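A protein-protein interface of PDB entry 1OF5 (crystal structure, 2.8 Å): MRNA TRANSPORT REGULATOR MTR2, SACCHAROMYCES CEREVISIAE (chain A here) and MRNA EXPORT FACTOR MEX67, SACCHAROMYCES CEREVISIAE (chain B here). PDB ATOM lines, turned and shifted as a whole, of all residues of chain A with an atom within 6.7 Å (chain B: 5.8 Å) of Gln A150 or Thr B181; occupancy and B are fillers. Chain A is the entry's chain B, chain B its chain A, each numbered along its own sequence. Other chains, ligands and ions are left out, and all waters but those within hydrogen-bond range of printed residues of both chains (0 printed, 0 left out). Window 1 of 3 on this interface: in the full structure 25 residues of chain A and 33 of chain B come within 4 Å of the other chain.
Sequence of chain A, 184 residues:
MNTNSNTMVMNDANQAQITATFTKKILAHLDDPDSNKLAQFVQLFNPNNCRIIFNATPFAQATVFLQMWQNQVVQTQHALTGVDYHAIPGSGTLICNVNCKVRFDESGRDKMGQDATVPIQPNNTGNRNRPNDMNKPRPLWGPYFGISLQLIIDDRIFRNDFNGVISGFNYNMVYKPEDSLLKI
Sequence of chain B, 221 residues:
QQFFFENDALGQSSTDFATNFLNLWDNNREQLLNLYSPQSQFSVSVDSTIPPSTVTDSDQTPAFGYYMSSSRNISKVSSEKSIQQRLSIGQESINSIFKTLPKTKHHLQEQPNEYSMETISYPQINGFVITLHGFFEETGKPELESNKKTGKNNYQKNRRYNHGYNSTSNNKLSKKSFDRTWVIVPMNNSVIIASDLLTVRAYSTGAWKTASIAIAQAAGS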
ATOM      1  N   HIS A  86      12.595   5.865 -24.181  1.00  0.00           N
ATOM      2  CA  HIS A  86      13.380   4.828 -24.815  1.00  0.00           C
ATOM      3  C   HIS A  86      12.885   3.523 -24.235  1.00  0.00           C
ATOM      4  O   HIS A  86      12.600   3.441 -23.038  1.00  0.00           O
ATOM      5  CB  HIS A  86      14.858   4.978 -24.464  1.00  0.00           C
ATOM      6  CG  HIS A  86      15.525   6.151 -25.107  1.00  0.00           C
ATOM      7  ND1 HIS A  86      16.758   6.614 -24.703  1.00  0.00           N
ATOM      8  CD2 HIS A  86      15.142   6.945 -26.134  1.00  0.00           C
ATOM      9  CE1 HIS A  86      17.106   7.647 -25.451  1.00  0.00           C
ATOM     10  NE2 HIS A  86      16.142   7.868 -26.327  1.00  0.00           N
ATOM     11  N   ILE A  95      11.601   3.973 -20.423  1.00  0.00           N
ATOM     12  CA  ILE A  95      11.798   5.090 -19.524  1.00  0.00           C
ATOM     13  C   ILE A  95      11.406   6.382 -20.222  1.00  0.00           C
ATOM     14  O   ILE A  95      11.798   6.643 -21.355  1.00  0.00           O
ATOM     15  CB  ILE A  95      13.271   5.164 -19.043  1.00  0.00           C
ATOM     16  CG1 ILE A  95      13.412   6.240 -17.954  1.00  0.00           C
ATOM     17  CG2 ILE A  95      14.204   5.428 -20.231  1.00  0.00           C
ATOM     18  CD1 ILE A  95      14.831   6.416 -17.450  1.00  0.00           C
ATOM     19  N   CYS A  96      10.614   7.181 -19.519  1.00  0.00           N
ATOM     20  CA  CYS A  96      10.131   8.441 -20.046  1.00  0.00           C
ATOM     21  C   CYS A  96      10.773   9.647 -19.376  1.00  0.00           C
ATOM     22  O   CYS A  96      10.992   9.664 -18.159  1.00  0.00           O
ATOM     23  CB  CYS A  96       8.621   8.513 -19.870  1.00  0.00           C
ATOM     24  SG  CYS A  96       7.774   7.049 -20.476  1.00  0.00           S
ATOM     25  N   ASN A  97      11.081  10.653 -20.185  1.00  0.00           N
ATOM     26  CA  ASN A  97      11.666  11.886 -19.684  1.00  0.00           C
ATOM     27  C   ASN A  97      10.617  12.955 -19.904  1.00  0.00           C
ATOM     28  O   ASN A  97      10.535  13.562 -20.976  1.00  0.00           O
ATOM     29  CB  ASN A  97      12.921  12.236 -20.453  1.00  0.00           C
ATOM     30  CG  ASN A  97      13.675  13.343 -19.808  1.00  0.00           C
ATOM     31  OD1 ASN A  97      13.829  13.355 -18.593  1.00  0.00           O
ATOM     32  ND2 ASN A  97      14.163  14.284 -20.607  1.00  0.00           N
ATOM     33  N   VAL A  98       9.811  13.186 -18.879  1.00  0.00           N
ATOM     34  CA  VAL A  98       8.727  14.135 -18.977  1.00  0.00           C
ATOM     35  C   VAL A  98       8.983  15.538 -18.447  1.00  0.00           C
ATOM     36  O   VAL A  98       9.834  15.759 -17.590  1.00  0.00           O
ATOM     37  CB  VAL A  98       7.504  13.522 -18.296  1.00  0.00           C
ATOM     38  CG1 VAL A  98       6.388  14.539 -18.152  1.00  0.00           C
ATOM     39  CG2 VAL A  98       7.051  12.317 -19.105  1.00  0.00           C
ATOM     40  N   ASN A  99       8.224  16.488 -18.989  1.00  0.00           N
ATOM     41  CA  ASN A  99       8.294  17.897 -18.607  1.00  0.00           C
ATOM     42  C   ASN A  99       6.890  18.513 -18.515  1.00  0.00           C
ATOM     43  O   ASN A  99       6.058  18.349 -19.411  1.00  0.00           O
ATOM     44  CB  ASN A  99       9.136  18.650 -19.621  1.00  0.00           C
ATOM     45  CG  ASN A  99      10.553  18.153 -19.652  1.00  0.00           C
ATOM     46  OD1 ASN A  99      11.398  18.597 -18.868  1.00  0.00           O
ATOM     47  ND2 ASN A  99      10.823  17.199 -20.542  1.00  0.00           N
ATOM     48  N   SER A 148      10.109  18.311 -13.700  1.00  0.00           N
ATOM     49  CA  SER A 148      10.821  17.346 -14.530  1.00  0.00           C
ATOM     50  C   SER A 148      10.414  15.984 -13.957  1.00  0.00           C
ATOM     51  O   SER A 148      10.421  15.782 -12.737  1.00  0.00           O
ATOM     52  CB  SER A 148      12.338  17.538 -14.421  1.00  0.00           C
ATOM     53  OG  SER A 148      13.014  16.688 -15.337  1.00  0.00           O
ATOM     54  N   LEU A 149      10.057  15.049 -14.827  1.00  0.00           N
ATOM     55  CA  LEU A 149       9.617  13.744 -14.357  1.00  0.00           C
ATOM     56  C   LEU A 149      10.063  12.582 -15.199  1.00  0.00           C
ATOM     57  O   LEU A 149       9.751  12.509 -16.388  1.00  0.00           O
ATOM     58  CB  LEU A 149       8.094  13.705 -14.274  1.00  0.00           C
ATOM     59  CG  LEU A 149       7.477  12.330 -13.996  1.00  0.00           C
ATOM     60  CD1 LEU A 149       7.952  11.810 -12.634  1.00  0.00           C
ATOM     61  CD2 LEU A 149       5.950  12.437 -14.046  1.00  0.00           C
ATOM     62  N   GLN A 150      10.784  11.661 -14.564  1.00  0.00           N
ATOM     63  CA  GLN A 150      11.242  10.447 -15.233  1.00  0.00           C
ATOM     64  C   GLN A 150      10.356   9.320 -14.700  1.00  0.00           C
ATOM     65  O   GLN A 150       9.935   9.354 -13.538  1.00  0.00           O
ATOM     66  CB  GLN A 150      12.700  10.148 -14.898  1.00  0.00           C
ATOM     67  CG  GLN A 150      13.697  11.189 -15.384  1.00  0.00           C
ATOM     68  CD  GLN A 150      13.518  12.530 -14.703  1.00  0.00           C
ATOM     69  OE1 GLN A 150      13.354  12.600 -13.480  1.00  0.00           O
ATOM     70  NE2 GLN A 150      13.552  13.608 -15.489  1.00  0.00           N
ATOM     71  N   LEU A 151      10.062   8.351 -15.561  1.00  0.00           N
ATOM     72  CA  LEU A 151       9.232   7.201 -15.207  1.00  0.00           C
ATOM     73  C   LEU A 151       9.753   5.941 -15.875  1.00  0.00           C
ATOM     74  O   LEU A 151      10.160   5.965 -17.046  1.00  0.00           O
ATOM     75  CB  LEU A 151       7.806   7.392 -15.700  1.00  0.00           C
ATOM     76  CG  LEU A 151       6.985   8.617 -15.325  1.00  0.00           C
ATOM     77  CD1 LEU A 151       5.822   8.743 -16.315  1.00  0.00           C
ATOM     78  CD2 LEU A 151       6.486   8.493 -13.892  1.00  0.00           C
ATOM     79  N   ILE A 152       9.746   4.840 -15.136  1.00  0.00           N
ATOM     80  CA  ILE A 152      10.160   3.570 -15.713  1.00  0.00           C
ATOM     81  C   ILE A 152       8.844   2.833 -15.799  1.00  0.00           C
ATOM     82  O   ILE A 152       8.150   2.677 -14.790  1.00  0.00           O
ATOM     83  CB  ILE A 152      11.159   2.824 -14.811  1.00  0.00           C
ATOM     84  CG1 ILE A 152      12.411   3.694 -14.630  1.00  0.00           C
ATOM     85  CG2 ILE A 152      11.526   1.491 -15.440  1.00  0.00           C
ATOM     86  CD1 ILE A 152      13.543   3.040 -13.909  1.00  0.00           C
ATOM     87  N   GLY A 168       9.281   3.266 -11.657  1.00  0.00           N
ATOM     88  CA  GLY A 168      10.159   4.420 -11.526  1.00  0.00           C
ATOM     89  C   GLY A 168       9.343   5.698 -11.477  1.00  0.00           C
ATOM     90  O   GLY A 168       8.496   5.945 -12.343  1.00  0.00           O
ATOM     91  N   PHE A 169       9.585   6.517 -10.460  1.00  0.00           N
ATOM     92  CA  PHE A 169       8.842   7.761 -10.314  1.00  0.00           C
ATOM     93  C   PHE A 169       9.732   8.870  -9.781  1.00  0.00           C
ATOM     94  O   PHE A 169       9.792   9.090  -8.575  1.00  0.00           O
ATOM     95  CB  PHE A 169       7.668   7.572  -9.350  1.00  0.00           C
ATOM     96  CG  PHE A 169       6.615   8.621  -9.481  1.00  0.00           C
ATOM     97  CD1 PHE A 169       5.711   8.579 -10.536  1.00  0.00           C
ATOM     98  CD2 PHE A 169       6.534   9.675  -8.570  1.00  0.00           C
ATOM     99  CE1 PHE A 169       4.736   9.578 -10.684  1.00  0.00           C
ATOM    100  CE2 PHE A 169       5.560  10.683  -8.710  1.00  0.00           C
ATOM    101  CZ  PHE A 169       4.666  10.632  -9.764  1.00  0.00           C
ATOM    102  N   ASN A 170      10.434   9.569 -10.662  1.00  0.00           N
ATOM    103  CA  ASN A 170      11.280  10.643 -10.190  1.00  0.00           C
ATOM    104  C   ASN A 170      10.620  11.943 -10.591  1.00  0.00           C
ATOM    105  O   ASN A 170      10.710  12.375 -11.749  1.00  0.00           O
ATOM    106  CB  ASN A 170      12.686  10.539 -10.776  1.00  0.00           C
ATOM    107  CG  ASN A 170      13.682  11.486 -10.096  1.00  0.00           C
ATOM    108  OD1 ASN A 170      13.491  11.906  -8.942  1.00  0.00           O
ATOM    109  ND2 ASN A 170      14.762  11.813 -10.807  1.00  0.00           N
ATOM    110  N   TYR A 171       9.947  12.544  -9.609  1.00  0.00           N
ATOM    111  CA  TYR A 171       9.213  13.792  -9.765  1.00  0.00           C
ATOM    112  C   TYR A 171       9.915  14.926  -9.045  1.00  0.00           C
ATOM    113  O   TYR A 171      10.020  14.900  -7.817  1.00  0.00           O
ATOM    114  CB  TYR A 171       7.849  13.624  -9.146  1.00  0.00           C
ATOM    115  CG  TYR A 171       6.909  14.774  -9.380  1.00  0.00           C
ATOM    116  CD1 TYR A 171       5.899  14.679 -10.333  1.00  0.00           C
ATOM    117  CD2 TYR A 171       6.975  15.925  -8.604  1.00  0.00           C
ATOM    118  CE1 TYR A 171       4.979  15.689 -10.495  1.00  0.00           C
ATOM    119  CE2 TYR A 171       6.053  16.950  -8.762  1.00  0.00           C
ATOM    120  CZ  TYR A 171       5.055  16.824  -9.708  1.00  0.00           C
ATOM    121  OH  TYR A 171       4.120  17.826  -9.869  1.00  0.00           O
ATOM    122  N   ASN A 172      10.376  15.931  -9.786  1.00  0.00           N
ATOM    123  CA  ASN A 172      11.068  17.058  -9.156  1.00  0.00           C
ATOM    124  C   ASN A 172      10.795  18.402  -9.782  1.00  0.00           C
ATOM    125  O   ASN A 172      10.845  18.553 -11.005  1.00  0.00           O
ATOM    126  CB  ASN A 172      12.574  16.840  -9.164  1.00  0.00           C
ATOM    127  CG  ASN A 172      12.985  15.699  -8.289  1.00  0.00           C
ATOM    128  OD1 ASN A 172      12.856  15.773  -7.065  1.00  0.00           O
ATOM    129  ND2 ASN A 172      13.468  14.616  -8.905  1.00  0.00           N
ATOM    130  N   GLU B 118      19.284  13.081  -8.879  1.00  0.00           N
ATOM    131  CA  GLU B 118      18.627  11.938  -8.278  1.00  0.00           C
ATOM    132  C   GLU B 118      19.178  10.684  -8.956  1.00  0.00           C
ATOM    133  O   GLU B 118      19.515  10.695 -10.155  1.00  0.00           O
ATOM    134  CB  GLU B 118      17.117  11.997  -8.485  1.00  0.00           C
ATOM    135  CG  GLU B 118      16.468  13.311  -8.115  1.00  0.00           C
ATOM    136  CD  GLU B 118      16.673  14.367  -9.169  1.00  0.00           C
ATOM    137  OE1 GLU B 118      16.604  14.025 -10.366  1.00  0.00           O
ATOM    138  OE2 GLU B 118      16.892  15.541  -8.801  1.00  0.00           O
ATOM    139  N   VAL B 129      19.595   4.764 -12.824  1.00  0.00           N
ATOM    140  CA  VAL B 129      19.165   5.922 -13.587  1.00  0.00           C
ATOM    141  C   VAL B 129      19.701   7.141 -12.875  1.00  0.00           C
ATOM    142  O   VAL B 129      19.435   7.348 -11.695  1.00  0.00           O
ATOM    143  CB  VAL B 129      17.631   6.047 -13.645  1.00  0.00           C
ATOM    144  CG1 VAL B 129      17.255   7.312 -14.407  1.00  0.00           C
ATOM    145  CG2 VAL B 129      17.035   4.839 -14.314  1.00  0.00           C
ATOM    146  N   ILE B 130      20.485   7.930 -13.583  1.00  0.00           N
ATOM    147  CA  ILE B 130      21.005   9.139 -12.990  1.00  0.00           C
ATOM    148  C   ILE B 130      20.414  10.291 -13.762  1.00  0.00           C
ATOM    149  O   ILE B 130      20.458  10.324 -14.999  1.00  0.00           O
ATOM    150  CB  ILE B 130      22.532   9.245 -13.076  1.00  0.00           C
ATOM    151  CG1 ILE B 130      23.188   8.078 -12.329  1.00  0.00           C
ATOM    152  CG2 ILE B 130      22.972  10.568 -12.478  1.00  0.00           C
ATOM    153  CD1 ILE B 130      24.700   8.159 -12.257  1.00  0.00           C
ATOM    154  N   THR B 131      19.825  11.218 -13.021  1.00  0.00           N
ATOM    155  CA  THR B 131      19.236  12.393 -13.620  1.00  0.00           C
ATOM    156  C   THR B 131      19.910  13.598 -13.024  1.00  0.00           C
ATOM    157  O   THR B 131      20.099  13.684 -11.800  1.00  0.00           O
ATOM    158  CB  THR B 131      17.750  12.496 -13.327  1.00  0.00           C
ATOM    159  OG1 THR B 131      17.050  11.526 -14.107  1.00  0.00           O
ATOM    160  CG2 THR B 131      17.245  13.881 -13.682  1.00  0.00           C
ATOM    161  N   LEU B 132      20.268  14.524 -13.903  1.00  0.00           N
ATOM    162  CA  LEU B 132      20.914  15.754 -13.495  1.00  0.00           C
ATOM    163  C   LEU B 132      20.151  16.978 -14.012  1.00  0.00           C
ATOM    164  O   LEU B 132      19.865  17.095 -15.211  1.00  0.00           O
ATOM    165  CB  LEU B 132      22.341  15.780 -14.017  1.00  0.00           C
ATOM    166  CG  LEU B 132      23.087  17.102 -13.837  1.00  0.00           C
ATOM    167  CD1 LEU B 132      23.287  17.389 -12.338  1.00  0.00           C
ATOM    168  CD2 LEU B 132      24.424  17.030 -14.585  1.00  0.00           C
ATOM    169  N   HIS B 133      19.817  17.876 -13.090  1.00  0.00           N
ATOM    170  CA  HIS B 133      19.116  19.115 -13.403  1.00  0.00           C
ATOM    171  C   HIS B 133      20.101  20.275 -13.197  1.00  0.00           C
ATOM    172  O   HIS B 133      20.875  20.277 -12.228  1.00  0.00           O
ATOM    173  CB  HIS B 133      17.924  19.283 -12.460  1.00  0.00           C
ATOM    174  CG  HIS B 133      17.035  18.079 -12.394  1.00  0.00           C
ATOM    175  ND1 HIS B 133      16.097  17.786 -13.365  1.00  0.00           N
ATOM    176  CD2 HIS B 133      16.951  17.082 -11.480  1.00  0.00           C
ATOM    177  CE1 HIS B 133      15.473  16.664 -13.051  1.00  0.00           C
ATOM    178  NE2 HIS B 133      15.971  16.216 -11.912  1.00  0.00           N
ATOM    179  N   ASP B 179      17.644  19.141 -18.193  1.00  0.00           N
ATOM    180  CA  ASP B 179      17.425  17.959 -17.360  1.00  0.00           C
ATOM    181  C   ASP B 179      17.924  16.805 -18.238  1.00  0.00           C
ATOM    182  O   ASP B 179      17.279  16.479 -19.254  1.00  0.00           O
ATOM    183  CB  ASP B 179      15.938  17.719 -17.074  1.00  0.00           C
ATOM    184  CG  ASP B 179      15.223  18.945 -16.539  1.00  0.00           C
ATOM    185  OD1 ASP B 179      15.622  19.492 -15.473  1.00  0.00           O
ATOM    186  OD2 ASP B 179      14.234  19.350 -17.194  1.00  0.00           O
ATOM    187  N   ARG B 180      19.062  16.205 -17.886  1.00  0.00           N
ATOM    188  CA  ARG B 180      19.573  15.074 -18.672  1.00  0.00           C
ATOM    189  C   ARG B 180      19.456  13.808 -17.829  1.00  0.00           C
ATOM    190  O   ARG B 180      19.789  13.815 -16.633  1.00  0.00           O
ATOM    191  CB  ARG B 180      21.028  15.292 -19.081  1.00  0.00           C
ATOM    192  CG  ARG B 180      21.497  14.328 -20.171  1.00  0.00           C
ATOM    193  CD  ARG B 180      22.795  14.801 -20.806  1.00  0.00           C
ATOM    194  NE  ARG B 180      23.177  14.029 -21.988  1.00  0.00           N
ATOM    195  CZ  ARG B 180      24.151  14.396 -22.826  1.00  0.00           C
ATOM    196  NH1 ARG B 180      24.828  15.520 -22.599  1.00  0.00           N
ATOM    197  NH2 ARG B 180      24.455  13.646 -23.889  1.00  0.00           N
ATOM    198  N   THR B 181      18.973  12.730 -18.441  1.00  0.00           N
ATOM    199  CA  THR B 181      18.796  11.471 -17.723  1.00  0.00           C
ATOM    200  C   THR B 181      19.551  10.301 -18.361  1.00  0.00           C
ATOM    201  O   THR B 181      19.210   9.850 -19.462  1.00  0.00           O
ATOM    202  CB  THR B 181      17.320  11.101 -17.655  1.00  0.00           C
ATOM    203  OG1 THR B 181      16.559  12.264 -17.304  1.00  0.00           O
ATOM    204  CG2 THR B 181      17.099  10.012 -16.617  1.00  0.00           C
ATOM    205  N   TRP B 182      20.567   9.806 -17.660  1.00  0.00           N
ATOM    206  CA  TRP B 182      21.349   8.691 -18.160  1.00  0.00           C
ATOM    207  C   TRP B 182      20.952   7.390 -17.488  1.00  0.00           C
ATOM    208  O   TRP B 182      20.949   7.287 -16.254  1.00  0.00           O
ATOM    209  CB  TRP B 182      22.828   8.908 -17.890  1.00  0.00           C
ATOM    210  CG  TRP B 182      23.408  10.125 -18.487  1.00  0.00           C
ATOM    211  CD1 TRP B 182      23.943  10.253 -19.729  1.00  0.00           C
ATOM    212  CD2 TRP B 182      23.568  11.392 -17.842  1.00  0.00           C
ATOM    213  NE1 TRP B 182      24.443  11.528 -19.902  1.00  0.00           N
ATOM    214  CE2 TRP B 182      24.227  12.246 -18.756  1.00  0.00           C
ATOM    215  CE3 TRP B 182      23.221  11.887 -16.576  1.00  0.00           C
ATOM    216  CZ2 TRP B 182      24.546  13.568 -18.451  1.00  0.00           C
ATOM    217  CZ3 TRP B 182      23.536  13.209 -16.265  1.00  0.00           C
ATOM    218  CH2 TRP B 182      24.196  14.034 -17.203  1.00  0.00           C
ATOM    219  N   VAL B 183      20.602   6.401 -18.303  1.00  0.00           N
ATOM    220  CA  VAL B 183      20.276   5.085 -17.799  1.00  0.00           C
ATOM    221  C   VAL B 183      21.580   4.326 -17.954  1.00  0.00           C
ATOM    222  O   VAL B 183      22.079   4.157 -19.068  1.00  0.00           O
ATOM    223  CB  VAL B 183      19.221   4.393 -18.632  1.00  0.00           C
ATOM    224  CG1 VAL B 183      19.295   2.875 -18.388  1.00  0.00           C
ATOM    225  CG2 VAL B 183      17.846   4.922 -18.248  1.00  0.00           C
ATOM    226  N   SER B 195      20.575   4.474 -22.135  1.00  0.00           N
ATOM    227  CA  SER B 195      19.712   5.557 -22.590  1.00  0.00           C
ATOM    228  C   SER B 195      20.210   6.937 -22.135  1.00  0.00           C
ATOM    229  O   SER B 195      20.647   7.112 -20.995  1.00  0.00           O
ATOM    230  CB  SER B 195      18.289   5.309 -22.087  1.00  0.00           C
ATOM    231  OG  SER B 195      17.522   6.490 -22.170  1.00  0.00           O
ATOM    232  N   ASP B 196      20.158   7.910 -23.042  1.00  0.00           N
ATOM    233  CA  ASP B 196      20.607   9.260 -22.739  1.00  0.00           C
ATOM    234  C   ASP B 196      19.525  10.217 -23.230  1.00  0.00           C
ATOM    235  O   ASP B 196      19.437  10.516 -24.426  1.00  0.00           O
ATOM    236  CB  ASP B 196      21.929   9.542 -23.448  1.00  0.00           C
ATOM    237  CG  ASP B 196      22.561  10.871 -23.022  1.00  0.00           C
ATOM    238  OD1 ASP B 196      21.812  11.803 -22.635  1.00  0.00           O
ATOM    239  OD2 ASP B 196      23.812  10.992 -23.093  1.00  0.00           O
ATOM    240  N   LEU B 197      18.690  10.676 -22.302  1.00  0.00           N
ATOM    241  CA  LEU B 197      17.593  11.582 -22.624  1.00  0.00           C
ATOM    242  C   LEU B 197      17.874  13.006 -22.153  1.00  0.00           C
ATOM    243  O   LEU B 197      17.839  13.297 -20.948  1.00  0.00           O
ATOM    244  CB  LEU B 197      16.279  11.063 -22.007  1.00  0.00           C
ATOM    245  CG  LEU B 197      15.790   9.730 -22.604  1.00  0.00           C
ATOM    246  CD1 LEU B 197      14.757   9.085 -21.714  1.00  0.00           C
ATOM    247  CD2 LEU B 197      15.212   9.951 -23.990  1.00  0.00           C
ATOM    248  N   LEU B 198      18.168  13.888 -23.111  1.00  0.00           N
ATOM    249  CA  LEU B 198      18.440  15.287 -22.808  1.00  0.00           C
ATOM    250  C   LEU B 198      17.245  16.188 -23.154  1.00  0.00           C
ATOM    251  O   LEU B 198      16.605  16.036 -24.197  1.00  0.00           O
ATOM    252  CB  LEU B 198      19.689  15.758 -23.562  1.00  0.00           C
ATOM    253  CG  LEU B 198      20.042  17.253 -23.531  1.00  0.00           C
ATOM    254  CD1 LEU B 198      19.969  17.819 -22.108  1.00  0.00           C
ATOM    255  CD2 LEU B 198      21.434  17.431 -24.091  1.00  0.00           C
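The side-chain carboxylate of Glu B118 lies within hydrogen-bond range of the side-chain amide nitrogen of Asn A170, at 2.9 Å.
OD2 of Asp B179 sits close to OD1 of Asn A99 (3.4 Å).
The side-chain hydroxyl (OG) of Ser A148 lies close to the side-chain carboxylate (OD2) of Asp B179, at 3.5 Å.
The side-chain hydroxyl (OG1) of Thr B181 sits at hydrogen-bond distance from the side-chain amide oxygen (OD1) of Asn A97, 3.2 Å away.
The side-chain hydroxyl of Ser B195 sits at hydrogen-bond distance from a ring nitrogen (ND1) of His A86 (2.6 Å).
The side-chain hydroxyl (OG1) of Thr B181 lies close to the side-chain hydroxyl (OG1) of Thr B131, at 3.3 Å.
A ring nitrogen (ND1) of His B133 is in hydrogen-bond range of the side-chain carboxylate of Asp B179 (2.8 Å).
NE of Arg B180 is in salt-bridge range of OD1 of Asp B196 (2.7 Å).
The indole nitrogen (NE1) of Trp B182 sits at hydrogen-bond distance from the side-chain carboxylate (OD2) of Asp B196, 3.3 Å away.
N of Val B183 is in hydrogen-bond range of O of Ser B195, 2.8 Å away.
The backbone NH of Ser A148 sits at hydrogen-bond distance from the backbone carbonyl oxygen of Asn A172.
Asp B196 touches His A86.
Val B129 touches Ile A95.
CG2 of Val B183 touches CD1 of Ile A95, 3.5 Å away.
Ile A95 touches Leu B197.
Asn A97 touches Leu B197.
Ser A148 touches His B133.
Thr B181 touches Gln A150.
Ile A152 touches Val B129 (CD1 to CG2, 3.9 Å).
Thr B131 touches Asn A170.
CD of Glu B118 touches ND2 of Asn A172 (3.2 Å).
Of chain B, only Thr B131 and Thr B181 come within 4 Å of Gln A150.
Printed residues of chain A within 4 Å of Val B183: Ile A95.
Printed residues of chain B within 4 Å of Asn A99: Asp B179 (3.4 Å).
Cys A96 touches none of the printed residues of chain B.
The nearest residue of chain B that does not touch Gln A150 is His B133 (4.4 Å).
The nearest residue of chain A that does not touch Thr B181 is Ile A95 (4.3 Å).
Hydrophobic or aromatic side chains of chain B within 4 Å of the printed part of chain A: Val B129, His B133, Val B183 and Leu B197.
Of the 16 printed residues of chain A, 9 touch a printed residue of chain B.
Among the printed residues, 18 pairs touch across the chains.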
